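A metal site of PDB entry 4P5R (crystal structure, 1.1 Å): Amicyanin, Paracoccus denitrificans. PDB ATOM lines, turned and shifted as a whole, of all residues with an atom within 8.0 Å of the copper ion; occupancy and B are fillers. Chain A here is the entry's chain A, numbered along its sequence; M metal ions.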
ATOM      1  N   ILE A  25      -8.913  20.535 -16.240  1.00  0.00           N
ATOM      2  CA  ILE A  25      -9.507  19.310 -15.782  1.00  0.00           C
ATOM      3  C   ILE A  25      -9.378  19.303 -14.268  1.00  0.00           C
ATOM      4  O   ILE A  25      -8.264  19.437 -13.730  1.00  0.00           O
ATOM      5  CB  ILE A  25      -8.825  18.066 -16.366  1.00  0.00           C
ATOM      6  CG1 ILE A  25      -8.563  18.193 -17.853  1.00  0.00           C
ATOM      7  CG2 ILE A  25      -9.685  16.845 -16.058  1.00  0.00           C
ATOM      8  CD1 ILE A  25      -7.773  17.029 -18.440  1.00  0.00           C
ATOM      9  N   MET A  28     -12.716  15.614 -11.449  1.00  0.00           N
ATOM     10  CA  MET A  28     -13.177  14.531 -12.311  1.00  0.00           C
ATOM     11  C   MET A  28     -14.074  14.993 -13.428  1.00  0.00           C
ATOM     12  O   MET A  28     -14.954  14.245 -13.906  1.00  0.00           O
ATOM     13  CB  MET A  28     -13.857  13.411 -11.515  1.00  0.00           C
ATOM     14  CG  MET A  28     -13.004  12.851 -10.381  1.00  0.00           C
ATOM     15  SD  MET A  28     -11.448  12.124 -10.838  1.00  0.00           S
ATOM     16  CE  MET A  28     -12.041  10.767 -11.731  1.00  0.00           C
ATOM     17  N   LYS A  29     -13.815  16.205 -13.922  1.00  0.00           N
ATOM     18  CA  LYS A  29     -14.585  16.760 -15.037  1.00  0.00           C
ATOM     19  C   LYS A  29     -13.697  17.613 -15.924  1.00  0.00           C
ATOM     20  O   LYS A  29     -12.784  18.312 -15.449  1.00  0.00           O
ATOM     21  CB  LYS A  29     -15.724  17.663 -14.497  1.00  0.00           C
ATOM     22  CG  LYS A  29     -16.759  16.976 -13.611  1.00  0.00           C
ATOM     23  CD  LYS A  29     -17.648  18.003 -12.886  1.00  0.00           C
ATOM     24  CE  LYS A  29     -18.180  17.443 -11.591  1.00  0.00           C
ATOM     25  NZ  LYS A  29     -19.126  18.433 -10.993  1.00  0.00           N
ATOM     26  N   TYR A  30     -13.998  17.622 -17.222  1.00  0.00           N
ATOM     27  CA  TYR A  30     -13.464  18.623 -18.107  1.00  0.00           C
ATOM     28  C   TYR A  30     -14.243  19.905 -17.809  1.00  0.00           C
ATOM     29  O   TYR A  30     -15.482  19.933 -17.911  1.00  0.00           O
ATOM     30  CB  TYR A  30     -13.619  18.193 -19.560  1.00  0.00           C
ATOM     31  CG  TYR A  30     -12.908  16.908 -19.902  1.00  0.00           C
ATOM     32  CD1 TYR A  30     -11.513  16.844 -19.956  1.00  0.00           C
ATOM     33  CD2 TYR A  30     -13.621  15.767 -20.177  1.00  0.00           C
ATOM     34  CE1 TYR A  30     -10.869  15.667 -20.287  1.00  0.00           C
ATOM     35  CE2 TYR A  30     -13.004  14.566 -20.538  1.00  0.00           C
ATOM     36  CZ  TYR A  30     -11.594  14.517 -20.595  1.00  0.00           C
ATOM     37  OH  TYR A  30     -11.033  13.363 -21.002  1.00  0.00           O
ATOM     38  N   ASN A  47      -4.316  19.269 -16.692  1.00  0.00           N
ATOM     39  CA  ASN A  47      -4.822  18.572 -15.543  1.00  0.00           C
ATOM     40  C   ASN A  47      -4.475  19.356 -14.281  1.00  0.00           C
ATOM     41  O   ASN A  47      -3.290  19.597 -13.989  1.00  0.00           O
ATOM     42  CB  ASN A  47      -4.242  17.165 -15.479  1.00  0.00           C
ATOM     43  CG  ASN A  47      -4.923  16.355 -14.398  1.00  0.00           C
ATOM     44  OD1 ASN A  47      -5.915  16.825 -13.784  1.00  0.00           O
ATOM     45  ND2 ASN A  47      -4.426  15.144 -14.127  1.00  0.00           N
ATOM     46  N   GLU A  49      -5.682  18.419 -11.197  1.00  0.00           N
ATOM     47  CA  GLU A  49      -5.899  17.647 -10.016  1.00  0.00           C
ATOM     48  C   GLU A  49      -4.982  16.447  -9.957  1.00  0.00           C
ATOM     49  O   GLU A  49      -4.300  16.026 -10.914  1.00  0.00           O
ATOM     50  CB  GLU A  49      -7.361  17.278  -9.834  1.00  0.00           C
ATOM     51  CG  GLU A  49      -7.745  16.304 -10.856  1.00  0.00           C
ATOM     52  CD  GLU A  49      -9.213  15.792 -10.624  1.00  0.00           C
ATOM     53  OE1 GLU A  49      -9.682  15.653  -9.522  1.00  0.00           O
ATOM     54  OE2 GLU A  49      -9.948  15.503 -11.511  1.00  0.00           O
ATOM     55  N   MET A  51      -5.517  13.246  -9.527  1.00  0.00           N
ATOM     56  CA  MET A  51      -5.887  12.080 -10.329  1.00  0.00           C
ATOM     57  C   MET A  51      -5.414  12.269 -11.768  1.00  0.00           C
ATOM     58  O   MET A  51      -5.793  13.240 -12.412  1.00  0.00           O
ATOM     59  CB  MET A  51      -7.422  11.996 -10.328  1.00  0.00           C
ATOM     60  CG  MET A  51      -8.011  10.942 -11.207  1.00  0.00           C
ATOM     61  SD  MET A  51      -7.595   9.306 -10.632  1.00  0.00           S
ATOM     62  CE  MET A  51      -8.881   9.272  -9.338  1.00  0.00           C
ATOM     63  N   PRO A  52      -4.678  11.301 -12.356  1.00  0.00           N
ATOM     64  CA  PRO A  52      -4.313  11.443 -13.767  1.00  0.00           C
ATOM     65  C   PRO A  52      -5.481  11.290 -14.704  1.00  0.00           C
ATOM     66  O   PRO A  52      -6.384  10.478 -14.473  1.00  0.00           O
ATOM     67  CB  PRO A  52      -3.257  10.331 -13.980  1.00  0.00           C
ATOM     68  CG  PRO A  52      -2.731  10.094 -12.579  1.00  0.00           C
ATOM     69  CD  PRO A  52      -3.937  10.211 -11.696  1.00  0.00           C
ATOM     70  N   HIS A  53      -5.459  12.057 -15.796  1.00  0.00           N
ATOM     71  CA  HIS A  53      -6.487  12.041 -16.836  1.00  0.00           C
ATOM     72  C   HIS A  53      -5.849  12.140 -18.192  1.00  0.00           C
ATOM     73  O   HIS A  53      -4.726  12.631 -18.316  1.00  0.00           O
ATOM     74  CB  HIS A  53      -7.436  13.252 -16.705  1.00  0.00           C
ATOM     75  CG  HIS A  53      -8.167  13.340 -15.391  1.00  0.00           C
ATOM     76  ND1 HIS A  53      -9.159  12.435 -15.036  1.00  0.00           N
ATOM     77  CD2 HIS A  53      -8.082  14.282 -14.398  1.00  0.00           C
ATOM     78  CE1 HIS A  53      -9.613  12.798 -13.861  1.00  0.00           C
ATOM     79  NE2 HIS A  53      -8.999  13.915 -13.467  1.00  0.00           N
ATOM     80  N   ASN A  54      -6.586  11.722 -19.229  1.00  0.00           N
ATOM     81  CA  ASN A  54      -6.175  11.998 -20.592  1.00  0.00           C
ATOM     82  C   ASN A  54      -7.369  12.502 -21.396  1.00  0.00           C
ATOM     83  O   ASN A  54      -8.431  12.793 -20.817  1.00  0.00           O
ATOM     84  CB  ASN A  54      -5.513  10.784 -21.265  1.00  0.00           C
ATOM     85  CG  ASN A  54      -6.492   9.691 -21.623  1.00  0.00           C
ATOM     86  OD1 ASN A  54      -7.610   9.671 -21.104  1.00  0.00           O
ATOM     87  ND2 ASN A  54      -6.121   8.826 -22.547  1.00  0.00           N
ATOM     88  N   VAL A  55      -7.170  12.607 -22.711  1.00  0.00           N
ATOM     89  CA  VAL A  55      -8.238  12.770 -23.668  1.00  0.00           C
ATOM     90  C   VAL A  55      -8.125  11.661 -24.705  1.00  0.00           C
ATOM     91  O   VAL A  55      -7.003  11.306 -25.095  1.00  0.00           O
ATOM     92  CB  VAL A  55      -8.245  14.161 -24.343  1.00  0.00           C
ATOM     93  CG1 VAL A  55      -8.562  15.241 -23.283  1.00  0.00           C
ATOM     94  CG2 VAL A  55      -7.004  14.485 -25.091  1.00  0.00           C
ATOM     95  N   MET A  71      -1.467  10.046 -20.565  1.00  0.00           N
ATOM     96  CA  MET A  71      -1.930  10.392 -19.227  1.00  0.00           C
ATOM     97  C   MET A  71      -1.155  11.620 -18.744  1.00  0.00           C
ATOM     98  O   MET A  71       0.078  11.698 -18.825  1.00  0.00           O
ATOM     99  CB  MET A  71      -1.738   9.252 -18.260  1.00  0.00           C
ATOM    100  CG  MET A  71      -2.557   7.977 -18.605  1.00  0.00           C
ATOM    101  SD  MET A  71      -4.297   8.251 -18.820  1.00  0.00           S
ATOM    102  CE  MET A  71      -4.757   8.955 -17.244  1.00  0.00           C
ATOM    103  N   MET A  72      -1.910  12.584 -18.221  1.00  0.00           N
ATOM    104  CA  MET A  72      -1.367  13.811 -17.648  1.00  0.00           C
ATOM    105  C   MET A  72      -1.417  13.699 -16.132  1.00  0.00           C
ATOM    106  O   MET A  72      -2.503  13.500 -15.565  1.00  0.00           O
ATOM    107  CB  MET A  72      -2.245  15.029 -18.054  1.00  0.00           C
ATOM    108  CG  MET A  72      -2.150  15.443 -19.495  1.00  0.00           C
ATOM    109  SD  MET A  72      -3.342  16.726 -19.970  1.00  0.00           S
ATOM    110  CE  MET A  72      -4.616  15.581 -20.316  1.00  0.00           C
ATOM    111  N   HIS A  91     -13.309  11.453 -24.478  1.00  0.00           N
ATOM    112  CA  HIS A  91     -13.532  11.014 -23.125  1.00  0.00           C
ATOM    113  C   HIS A  91     -12.193  10.759 -22.460  1.00  0.00           C
ATOM    114  O   HIS A  91     -11.140  10.756 -23.134  1.00  0.00           O
ATOM    115  CB  HIS A  91     -14.436   9.769 -23.075  1.00  0.00           C
ATOM    116  CG  HIS A  91     -13.802   8.542 -23.621  1.00  0.00           C
ATOM    117  ND1 HIS A  91     -13.755   8.248 -24.953  1.00  0.00           N
ATOM    118  CD2 HIS A  91     -13.149   7.523 -23.000  1.00  0.00           C
ATOM    119  CE1 HIS A  91     -13.121   7.103 -25.151  1.00  0.00           C
ATOM    120  NE2 HIS A  91     -12.718   6.652 -23.979  1.00  0.00           N
ATOM    121  N   CYS A  92     -12.228  10.447 -21.170  1.00  0.00           N
ATOM    122  CA  CYS A  92     -11.013  10.087 -20.438  1.00  0.00           C
ATOM    123  C   CYS A  92     -10.927   8.551 -20.401  1.00  0.00           C
ATOM    124  O   CYS A  92     -11.877   7.893 -19.977  1.00  0.00           O
ATOM    125  CB  CYS A  92     -11.080  10.669 -19.031  1.00  0.00           C
ATOM    126  SG  CYS A  92      -9.606  10.164 -18.099  1.00  0.00           S
ATOM    127  N   THR A  93      -9.818   7.980 -20.842  1.00  0.00           N
ATOM    128  CA  THR A  93      -9.686   6.546 -20.960  1.00  0.00           C
ATOM    129  C   THR A  93      -9.984   5.819 -19.632  1.00  0.00           C
ATOM    130  O   THR A  93     -10.823   4.934 -19.610  1.00  0.00           O
ATOM    131  CB  THR A  93      -8.308   6.134 -21.541  1.00  0.00           C
ATOM    132  OG1 THR A  93      -8.152   6.773 -22.797  1.00  0.00           O
ATOM    133  CG2 THR A  93      -8.201   4.641 -21.665  1.00  0.00           C
ATOM    134  N   PRO A  94      -9.296   6.148 -18.509  1.00  0.00           N
ATOM    135  CA  PRO A  94      -9.631   5.421 -17.283  1.00  0.00           C
ATOM    136  C   PRO A  94     -10.988   5.821 -16.694  1.00  0.00           C
ATOM    137  O   PRO A  94     -11.522   5.064 -15.879  1.00  0.00           O
ATOM    138  CB  PRO A  94      -8.516   5.842 -16.307  1.00  0.00           C
ATOM    139  CG  PRO A  94      -8.008   7.171 -16.844  1.00  0.00           C
ATOM    140  CD  PRO A  94      -8.101   6.998 -18.351  1.00  0.00           C
ATOM    141  N   HIS A  95     -11.498   7.002 -17.044  1.00  0.00           N
ATOM    142  CA  HIS A  95     -12.719   7.547 -16.462  1.00  0.00           C
ATOM    143  C   HIS A  95     -13.701   7.910 -17.575  1.00  0.00           C
ATOM    144  O   HIS A  95     -13.949   9.084 -17.836  1.00  0.00           O
ATOM    145  CB  HIS A  95     -12.417   8.805 -15.667  1.00  0.00           C
ATOM    146  CG  HIS A  95     -11.322   8.643 -14.678  1.00  0.00           C
ATOM    147  ND1 HIS A  95     -10.210   9.463 -14.691  1.00  0.00           N
ATOM    148  CD2 HIS A  95     -11.162   7.758 -13.665  1.00  0.00           C
ATOM    149  CE1 HIS A  95      -9.416   9.077 -13.716  1.00  0.00           C
ATOM    150  NE2 HIS A  95      -9.970   8.048 -13.068  1.00  0.00           N
ATOM    151  N   PRO A  96     -14.308   6.904 -18.246  1.00  0.00           N
ATOM    152  CA  PRO A  96     -15.100   7.202 -19.447  1.00  0.00           C
ATOM    153  C   PRO A  96     -16.432   7.898 -19.175  1.00  0.00           C
ATOM    154  O   PRO A  96     -17.092   8.348 -20.113  1.00  0.00           O
ATOM    155  CB  PRO A  96     -15.246   5.833 -20.124  1.00  0.00           C
ATOM    156  CG  PRO A  96     -15.131   4.879 -18.996  1.00  0.00           C
ATOM    157  CD  PRO A  96     -14.039   5.477 -18.149  1.00  0.00           C
ATOM    158  N   PHE A  97     -16.800   8.060 -17.909  1.00  0.00           N
ATOM    159  CA  PHE A  97     -17.894   8.937 -17.523  1.00  0.00           C
ATOM    160  C   PHE A  97     -17.519  10.419 -17.723  1.00  0.00           C
ATOM    161  O   PHE A  97     -18.427  11.261 -17.726  1.00  0.00           O
ATOM    162  CB  PHE A  97     -18.310   8.668 -16.064  1.00  0.00           C
ATOM    163  CG  PHE A  97     -17.178   8.711 -15.082  1.00  0.00           C
ATOM    164  CD1 PHE A  97     -16.700   9.937 -14.618  1.00  0.00           C
ATOM    165  CD2 PHE A  97     -16.568   7.553 -14.627  1.00  0.00           C
ATOM    166  CE1 PHE A  97     -15.630   9.967 -13.701  1.00  0.00           C
ATOM    167  CE2 PHE A  97     -15.537   7.572 -13.726  1.00  0.00           C
ATOM    168  CZ  PHE A  97     -15.037   8.787 -13.255  1.00  0.00           C
ATOM    169  N   MET A  98     -16.234  10.739 -17.920  1.00  0.00           N
ATOM    170  CA  MET A  98     -15.765  12.113 -18.250  1.00  0.00           C
ATOM    171  C   MET A  98     -15.825  12.251 -19.747  1.00  0.00           C
ATOM    172  O   MET A  98     -15.073  11.583 -20.468  1.00  0.00           O
ATOM    173  CB  MET A  98     -14.326  12.325 -17.785  1.00  0.00           C
ATOM    174  CG  MET A  98     -14.143  12.211 -16.310  1.00  0.00           C
ATOM    175  SD  MET A  98     -12.429  12.379 -15.766  1.00  0.00           S
ATOM    176  CE  MET A  98     -12.020  14.036 -16.400  1.00  0.00           C
HETATM  177 CU    CU M   1      -9.799  10.876 -16.065  1.00  0.00          CU
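The copper ion is bound by ND1 of His 53 (2.0 Å), ND1 of His 95 (2.0 Å) and SG of Cys 92 (2.2 Å).
Slightly farther from the copper ion lies SD of Met 98 (3.0 Å).
ND1 of His 53 sits close to SD of Met 98, 3.4 Å away.
A ring nitrogen (NE2) of His 53 lies close to the backbone carbonyl oxygen of Met 51 (3.4 Å).
OE2 of Glu 49 sits at hydrogen-bond distance from NE2 of His 53, 2.7 Å away.
The backbone carbonyl oxygen (O) of His 53 lies within hydrogen-bond range of the backbone NH (N) of Met 72 (2.8 Å).
NE2 of His 95 lies close to SD of Met 51.
O of Met 98 sits at hydrogen-bond distance from N of Cys 92 (3.1 Å).
The side-chain sulfur (SG) of Cys 92 sits close to the backbone NH (N) of Asn 54, 3.6 Å away.
The backbone NH (N) of Cys 92 is in hydrogen-bond range of the side-chain hydroxyl (OH) of Tyr 30, 3.2 Å away.
Pro 52 touches the copper ion (O to CU, 3.8 Å).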
